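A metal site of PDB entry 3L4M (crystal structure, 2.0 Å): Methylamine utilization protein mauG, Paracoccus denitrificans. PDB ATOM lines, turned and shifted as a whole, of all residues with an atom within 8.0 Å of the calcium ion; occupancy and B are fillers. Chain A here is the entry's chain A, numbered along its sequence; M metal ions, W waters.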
ATOM      1  N   ARG A  39       1.790 -38.484 -18.925  1.00  0.00           N
ATOM      2  CA  ARG A  39       0.877 -37.556 -19.624  1.00  0.00           C
ATOM      3  C   ARG A  39       1.546 -36.153 -19.846  1.00  0.00           C
ATOM      4  O   ARG A  39       0.939 -35.125 -19.691  1.00  0.00           O
ATOM      5  CB  ARG A  39      -0.517 -37.448 -18.961  1.00  0.00           C
ATOM      6  CG  ARG A  39      -1.694 -37.120 -20.054  1.00  0.00           C
ATOM      7  CD  ARG A  39      -3.231 -37.236 -19.703  1.00  0.00           C
ATOM      8  NE  ARG A  39      -3.566 -35.887 -19.568  1.00  0.00           N
ATOM      9  CZ  ARG A  39      -4.360 -35.026 -20.210  1.00  0.00           C
ATOM     10  NH1 ARG A  39      -5.434 -35.219 -21.039  1.00  0.00           N
ATOM     11  NH2 ARG A  39      -4.082 -33.830 -19.782  1.00  0.00           N
ATOM     12  N   THR A  42       1.125 -33.659 -16.853  1.00  0.00           N
ATOM     13  CA  THR A  42      -0.161 -33.047 -16.496  1.00  0.00           C
ATOM     14  C   THR A  42      -1.042 -34.157 -15.841  1.00  0.00           C
ATOM     15  O   THR A  42      -0.607 -35.320 -15.686  1.00  0.00           O
ATOM     16  CB  THR A  42      -0.862 -32.534 -17.750  1.00  0.00           C
ATOM     17  OG1 THR A  42      -1.159 -33.665 -18.602  1.00  0.00           O
ATOM     18  CG2 THR A  42      -0.028 -31.554 -18.482  1.00  0.00           C
ATOM     19  N   ASP A  43      -2.263 -33.794 -15.511  1.00  0.00           N
ATOM     20  CA  ASP A  43      -3.172 -34.588 -14.675  1.00  0.00           C
ATOM     21  C   ASP A  43      -4.223 -35.356 -15.484  1.00  0.00           C
ATOM     22  O   ASP A  43      -5.176 -34.737 -15.975  1.00  0.00           O
ATOM     23  CB  ASP A  43      -3.832 -33.686 -13.592  1.00  0.00           C
ATOM     24  CG  ASP A  43      -4.469 -34.507 -12.440  1.00  0.00           C
ATOM     25  OD1 ASP A  43      -4.938 -33.872 -11.466  1.00  0.00           O
ATOM     26  OD2 ASP A  43      -4.541 -35.772 -12.539  1.00  0.00           O
ATOM     27  N   LEU A  51     -11.321 -33.008 -16.557  1.00  0.00           N
ATOM     28  CA  LEU A  51      -9.877 -32.836 -16.373  1.00  0.00           C
ATOM     29  C   LEU A  51      -9.492 -31.364 -16.270  1.00  0.00           C
ATOM     30  O   LEU A  51      -8.299 -31.044 -16.304  1.00  0.00           O
ATOM     31  CB  LEU A  51      -9.066 -33.471 -17.528  1.00  0.00           C
ATOM     32  CG  LEU A  51      -8.675 -34.942 -17.352  1.00  0.00           C
ATOM     33  CD1 LEU A  51      -9.906 -35.731 -17.100  1.00  0.00           C
ATOM     34  CD2 LEU A  51      -7.954 -35.499 -18.612  1.00  0.00           C
ATOM     35  N   ALA A  52     -10.477 -30.478 -16.111  1.00  0.00           N
ATOM     36  CA  ALA A  52     -10.201 -29.034 -16.067  1.00  0.00           C
ATOM     37  C   ALA A  52      -9.352 -28.618 -14.861  1.00  0.00           C
ATOM     38  O   ALA A  52      -8.461 -27.819 -15.033  1.00  0.00           O
ATOM     39  CB  ALA A  52     -11.500 -28.201 -16.149  1.00  0.00           C
ATOM     40  N   ASN A  66      -6.172 -24.987 -14.398  1.00  0.00           N
ATOM     41  CA  ASN A  66      -5.751 -26.258 -14.976  1.00  0.00           C
ATOM     42  C   ASN A  66      -4.249 -26.511 -14.667  1.00  0.00           C
ATOM     43  O   ASN A  66      -3.429 -25.576 -14.714  1.00  0.00           O
ATOM     44  CB  ASN A  66      -5.972 -26.136 -16.490  1.00  0.00           C
ATOM     45  CG  ASN A  66      -5.636 -27.401 -17.243  1.00  0.00           C
ATOM     46  OD1 ASN A  66      -4.667 -27.417 -18.027  1.00  0.00           O
ATOM     47  ND2 ASN A  66      -6.365 -28.495 -16.960  1.00  0.00           N
ATOM     48  N   THR A  67      -3.924 -27.764 -14.339  1.00  0.00           N
ATOM     49  CA  THR A  67      -2.545 -28.136 -14.010  1.00  0.00           C
ATOM     50  C   THR A  67      -1.671 -28.089 -15.311  1.00  0.00           C
ATOM     51  O   THR A  67      -1.931 -28.793 -16.237  1.00  0.00           O
ATOM     52  CB  THR A  67      -2.504 -29.547 -13.456  1.00  0.00           C
ATOM     53  OG1 THR A  67      -3.123 -29.582 -12.185  1.00  0.00           O
ATOM     54  CG2 THR A  67      -1.096 -30.072 -13.283  1.00  0.00           C
ATOM     55  N   PRO A  68      -0.667 -27.234 -15.362  1.00  0.00           N
ATOM     56  CA  PRO A  68       0.062 -27.106 -16.644  1.00  0.00           C
ATOM     57  C   PRO A  68       1.189 -28.172 -16.742  1.00  0.00           C
ATOM     58  O   PRO A  68       1.594 -28.772 -15.745  1.00  0.00           O
ATOM     59  CB  PRO A  68       0.675 -25.697 -16.578  1.00  0.00           C
ATOM     60  CG  PRO A  68       0.918 -25.588 -15.035  1.00  0.00           C
ATOM     61  CD  PRO A  68      -0.255 -26.227 -14.372  1.00  0.00           C
ATOM     62  N   THR A  69       1.721 -28.364 -17.927  1.00  0.00           N
ATOM     63  CA  THR A  69       2.912 -29.219 -18.103  1.00  0.00           C
ATOM     64  C   THR A  69       4.135 -28.677 -17.458  1.00  0.00           C
ATOM     65  O   THR A  69       4.327 -27.469 -17.402  1.00  0.00           O
ATOM     66  CB  THR A  69       3.259 -29.500 -19.633  1.00  0.00           C
ATOM     67  OG1 THR A  69       4.359 -30.425 -19.685  1.00  0.00           O
ATOM     68  CG2 THR A  69       3.673 -28.219 -20.425  1.00  0.00           C
ATOM     69  N   TRP A  93       0.241 -19.744 -13.864  1.00  0.00           N
ATOM     70  CA  TRP A  93      -0.460 -19.067 -14.948  1.00  0.00           C
ATOM     71  C   TRP A  93      -0.487 -17.557 -14.716  1.00  0.00           C
ATOM     72  O   TRP A  93      -0.614 -16.811 -15.664  1.00  0.00           O
ATOM     73  CB  TRP A  93      -1.906 -19.550 -15.072  1.00  0.00           C
ATOM     74  CG  TRP A  93      -2.120 -20.923 -15.604  1.00  0.00           C
ATOM     75  CD1 TRP A  93      -2.319 -22.057 -14.875  1.00  0.00           C
ATOM     76  CD2 TRP A  93      -2.206 -21.321 -16.995  1.00  0.00           C
ATOM     77  NE1 TRP A  93      -2.511 -23.143 -15.727  1.00  0.00           N
ATOM     78  CE2 TRP A  93      -2.454 -22.710 -17.023  1.00  0.00           C
ATOM     79  CE3 TRP A  93      -2.116 -20.632 -18.208  1.00  0.00           C
ATOM     80  CZ2 TRP A  93      -2.607 -23.438 -18.233  1.00  0.00           C
ATOM     81  CZ3 TRP A  93      -2.292 -21.365 -19.444  1.00  0.00           C
ATOM     82  CH2 TRP A  93      -2.513 -22.733 -19.430  1.00  0.00           C
ATOM     83  N   ASN A 271       4.026 -30.165 -26.630  1.00  0.00           N
ATOM     84  CA  ASN A 271       3.146 -31.212 -26.126  1.00  0.00           C
ATOM     85  C   ASN A 271       1.645 -30.831 -26.070  1.00  0.00           C
ATOM     86  O   ASN A 271       0.845 -31.550 -25.470  1.00  0.00           O
ATOM     87  CB  ASN A 271       3.688 -31.711 -24.765  1.00  0.00           C
ATOM     88  CG  ASN A 271       4.962 -32.482 -24.948  1.00  0.00           C
ATOM     89  OD1 ASN A 271       5.035 -33.290 -25.897  1.00  0.00           O
ATOM     90  ND2 ASN A 271       5.976 -32.270 -24.053  1.00  0.00           N
ATOM     91  N   VAL A 272       1.283 -29.712 -26.690  1.00  0.00           N
ATOM     92  CA  VAL A 272      -0.075 -29.221 -26.561  1.00  0.00           C
ATOM     93  C   VAL A 272      -1.100 -30.283 -26.971  1.00  0.00           C
ATOM     94  O   VAL A 272      -2.233 -30.373 -26.387  1.00  0.00           O
ATOM     95  CB  VAL A 272      -0.313 -27.823 -27.258  1.00  0.00           C
ATOM     96  CG1 VAL A 272      -0.305 -27.923 -28.801  1.00  0.00           C
ATOM     97  CG2 VAL A 272      -1.652 -27.206 -26.805  1.00  0.00           C
ATOM     98  N   VAL A 274      -1.237 -33.325 -26.403  1.00  0.00           N
ATOM     99  CA  VAL A 274      -1.539 -34.347 -25.434  1.00  0.00           C
ATOM    100  C   VAL A 274      -1.828 -33.786 -24.028  1.00  0.00           C
ATOM    101  O   VAL A 274      -1.857 -34.550 -23.056  1.00  0.00           O
ATOM    102  CB  VAL A 274      -0.438 -35.462 -25.433  1.00  0.00           C
ATOM    103  CG1 VAL A 274      -0.279 -36.029 -26.801  1.00  0.00           C
ATOM    104  CG2 VAL A 274       0.917 -34.891 -24.945  1.00  0.00           C
ATOM    105  N   THR A 275      -2.017 -32.464 -23.883  1.00  0.00           N
ATOM    106  CA  THR A 275      -2.191 -31.902 -22.514  1.00  0.00           C
ATOM    107  C   THR A 275      -3.512 -31.153 -22.348  1.00  0.00           C
ATOM    108  O   THR A 275      -3.586 -30.190 -21.572  1.00  0.00           O
ATOM    109  CB  THR A 275      -1.054 -30.918 -22.151  1.00  0.00           C
ATOM    110  OG1 THR A 275      -1.006 -29.887 -23.161  1.00  0.00           O
ATOM    111  CG2 THR A 275       0.311 -31.645 -22.106  1.00  0.00           C
ATOM    112  N   GLY A 276      -4.525 -31.555 -23.126  1.00  0.00           N
ATOM    113  CA  GLY A 276      -5.891 -31.040 -22.998  1.00  0.00           C
ATOM    114  C   GLY A 276      -6.452 -31.392 -21.607  1.00  0.00           C
ATOM    115  O   GLY A 276      -5.972 -32.310 -20.927  1.00  0.00           O
ATOM    116  N   PRO A 277      -7.504 -30.695 -21.170  1.00  0.00           N
ATOM    117  CA  PRO A 277      -8.221 -29.584 -21.771  1.00  0.00           C
ATOM    118  C   PRO A 277      -7.346 -28.315 -21.721  1.00  0.00           C
ATOM    119  O   PRO A 277      -6.281 -28.286 -21.073  1.00  0.00           O
ATOM    120  CB  PRO A 277      -9.479 -29.454 -20.864  1.00  0.00           C
ATOM    121  CG  PRO A 277      -8.962 -29.865 -19.532  1.00  0.00           C
ATOM    122  CD  PRO A 277      -8.058 -31.040 -19.838  1.00  0.00           C
ATOM    123  N   TYR A 278      -7.801 -27.238 -22.360  1.00  0.00           N
ATOM    124  CA  TYR A 278      -6.910 -26.108 -22.617  1.00  0.00           C
ATOM    125  C   TYR A 278      -7.282 -24.811 -21.905  1.00  0.00           C
ATOM    126  O   TYR A 278      -8.426 -24.659 -21.518  1.00  0.00           O
ATOM    127  CB  TYR A 278      -6.908 -25.915 -24.141  1.00  0.00           C
ATOM    128  CG  TYR A 278      -6.411 -27.165 -24.796  1.00  0.00           C
ATOM    129  CD1 TYR A 278      -7.269 -28.041 -25.456  1.00  0.00           C
ATOM    130  CD2 TYR A 278      -5.056 -27.494 -24.708  1.00  0.00           C
ATOM    131  CE1 TYR A 278      -6.770 -29.232 -25.966  1.00  0.00           C
ATOM    132  CE2 TYR A 278      -4.553 -28.650 -25.291  1.00  0.00           C
ATOM    133  CZ  TYR A 278      -5.397 -29.489 -25.915  1.00  0.00           C
ATOM    134  OH  TYR A 278      -4.832 -30.626 -26.475  1.00  0.00           O
ATOM    135  N   MET A 279      -6.330 -23.883 -21.849  1.00  0.00           N
ATOM    136  CA  MET A 279      -6.431 -22.567 -21.215  1.00  0.00           C
ATOM    137  C   MET A 279      -6.254 -22.718 -19.713  1.00  0.00           C
ATOM    138  O   MET A 279      -6.169 -23.865 -19.182  1.00  0.00           O
ATOM    139  CB  MET A 279      -7.757 -21.879 -21.608  1.00  0.00           C
ATOM    140  CG  MET A 279      -7.928 -21.744 -23.179  1.00  0.00           C
ATOM    141  SD  MET A 279      -6.474 -20.906 -23.956  1.00  0.00           S
ATOM    142  CE  MET A 279      -6.973 -21.085 -25.679  1.00  0.00           C
ATOM    143  N   HIS A 280      -6.193 -21.582 -19.025  1.00  0.00           N
ATOM    144  CA  HIS A 280      -5.808 -21.530 -17.614  1.00  0.00           C
ATOM    145  C   HIS A 280      -6.849 -22.216 -16.752  1.00  0.00           C
ATOM    146  O   HIS A 280      -6.548 -22.653 -15.647  1.00  0.00           O
ATOM    147  CB  HIS A 280      -5.550 -20.066 -17.158  1.00  0.00           C
ATOM    148  CG  HIS A 280      -6.777 -19.202 -17.161  1.00  0.00           C
ATOM    149  ND1 HIS A 280      -7.066 -18.309 -18.183  1.00  0.00           N
ATOM    150  CD2 HIS A 280      -7.801 -19.106 -16.277  1.00  0.00           C
ATOM    151  CE1 HIS A 280      -8.211 -17.700 -17.928  1.00  0.00           C
ATOM    152  NE2 HIS A 280      -8.670 -18.156 -16.766  1.00  0.00           N
ATOM    153  N   ASN A 281      -8.080 -22.291 -17.261  1.00  0.00           N
ATOM    154  CA  ASN A 281      -9.206 -22.896 -16.535  1.00  0.00           C
ATOM    155  C   ASN A 281      -9.722 -24.208 -17.186  1.00  0.00           C
ATOM    156  O   ASN A 281     -10.797 -24.698 -16.846  1.00  0.00           O
ATOM    157  CB  ASN A 281     -10.359 -21.879 -16.337  1.00  0.00           C
ATOM    158  CG  ASN A 281     -10.843 -21.290 -17.641  1.00  0.00           C
ATOM    159  OD1 ASN A 281     -10.475 -21.763 -18.701  1.00  0.00           O
ATOM    160  ND2 ASN A 281     -11.654 -20.261 -17.578  1.00  0.00           N
ATOM    161  N   GLY A 282      -8.938 -24.761 -18.108  1.00  0.00           N
ATOM    162  CA  GLY A 282      -9.311 -26.027 -18.745  1.00  0.00           C
ATOM    163  C   GLY A 282     -10.660 -26.005 -19.437  1.00  0.00           C
ATOM    164  O   GLY A 282     -11.256 -27.065 -19.590  1.00  0.00           O
ATOM    165  N   VAL A 283     -11.106 -24.840 -19.916  1.00  0.00           N
ATOM    166  CA  VAL A 283     -12.526 -24.701 -20.394  1.00  0.00           C
ATOM    167  C   VAL A 283     -12.785 -25.391 -21.716  1.00  0.00           C
ATOM    168  O   VAL A 283     -13.912 -25.772 -21.988  1.00  0.00           O
ATOM    169  CB  VAL A 283     -12.901 -23.177 -20.454  1.00  0.00           C
ATOM    170  CG1 VAL A 283     -12.010 -22.374 -21.446  1.00  0.00           C
ATOM    171  CG2 VAL A 283     -14.406 -22.926 -20.734  1.00  0.00           C
ATOM    172  N   PHE A 284     -11.757 -25.577 -22.563  1.00  0.00           N
ATOM    173  CA  PHE A 284     -11.983 -26.250 -23.866  1.00  0.00           C
ATOM    174  C   PHE A 284     -11.322 -27.652 -23.836  1.00  0.00           C
ATOM    175  O   PHE A 284     -10.097 -27.732 -23.689  1.00  0.00           O
ATOM    176  CB  PHE A 284     -11.339 -25.413 -25.048  1.00  0.00           C
ATOM    177  CG  PHE A 284     -11.801 -23.966 -25.107  1.00  0.00           C
ATOM    178  CD1 PHE A 284     -13.128 -23.653 -24.892  1.00  0.00           C
ATOM    179  CD2 PHE A 284     -10.901 -22.934 -25.383  1.00  0.00           C
ATOM    180  CE1 PHE A 284     -13.547 -22.370 -24.920  1.00  0.00           C
ATOM    181  CE2 PHE A 284     -11.355 -21.618 -25.435  1.00  0.00           C
ATOM    182  CZ  PHE A 284     -12.653 -21.345 -25.202  1.00  0.00           C
HETATM  183 CA    CA M   1      -4.033 -28.341 -20.199  1.00  0.00          CA
HETATM  184  O   HOH W   1      -4.029 -25.858 -20.291  1.00  0.00           O
HETATM  185  O   HOH W   2      -2.544 -27.799 -22.089  1.00  0.00           O
HETATM  186  O   HOH W   3      -1.960 -28.675 -19.083  1.00  0.00           O
HETATM  187  O   HOH W   4      -4.754 -30.445 -18.876  1.00  0.00           O
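The backbone carbonyl oxygen of Val 272 lies within hydrogen-bond range of the side-chain hydroxyl of Thr 275 (3.5 Å).
The backbone carbonyl oxygen of Asn 271 is in hydrogen-bond range of the side-chain hydroxyl of Thr 275 (3.4 Å).
O of Asn 66 sits at hydrogen-bond distance from NE1 of Trp 93.
ND2 of Asn 66 sits at hydrogen-bond distance from O of Leu 51, 3.3 Å away.
ND2 of Asn 66 sits at hydrogen-bond distance from O of Ala 52 (2.9 Å).
The backbone carbonyl oxygen (O) of His 280 sits at hydrogen-bond distance from the backbone NH (N) of Asn 66 (2.7 Å).
Of the 23 residues printed, 3 come within 4 Å of the calcium ion.
The nearest printed residue that does not touch the calcium ion is Gly 276 (4.1 Å).
O of Thr 275 binds the calcium ion, 2.3 Å away.
Water W3 is bound to the calcium ion, at 2.4 Å.
O of Pro 277 binds the calcium ion (2.4 Å).
The side-chain amide oxygen (OD1) of Asn 66 binds the calcium ion, 2.4 Å away.
The calcium ion is bound by water W2, 2.5 Å away.
Water W1 is bound to the calcium ion (2.5 Å).
Water W4 is bound to the calcium ion, at 2.6 Å.
Water W4 bridges O of Gly 276 (3.0 Å) and ND2 of Asn 66 (3.2 Å).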
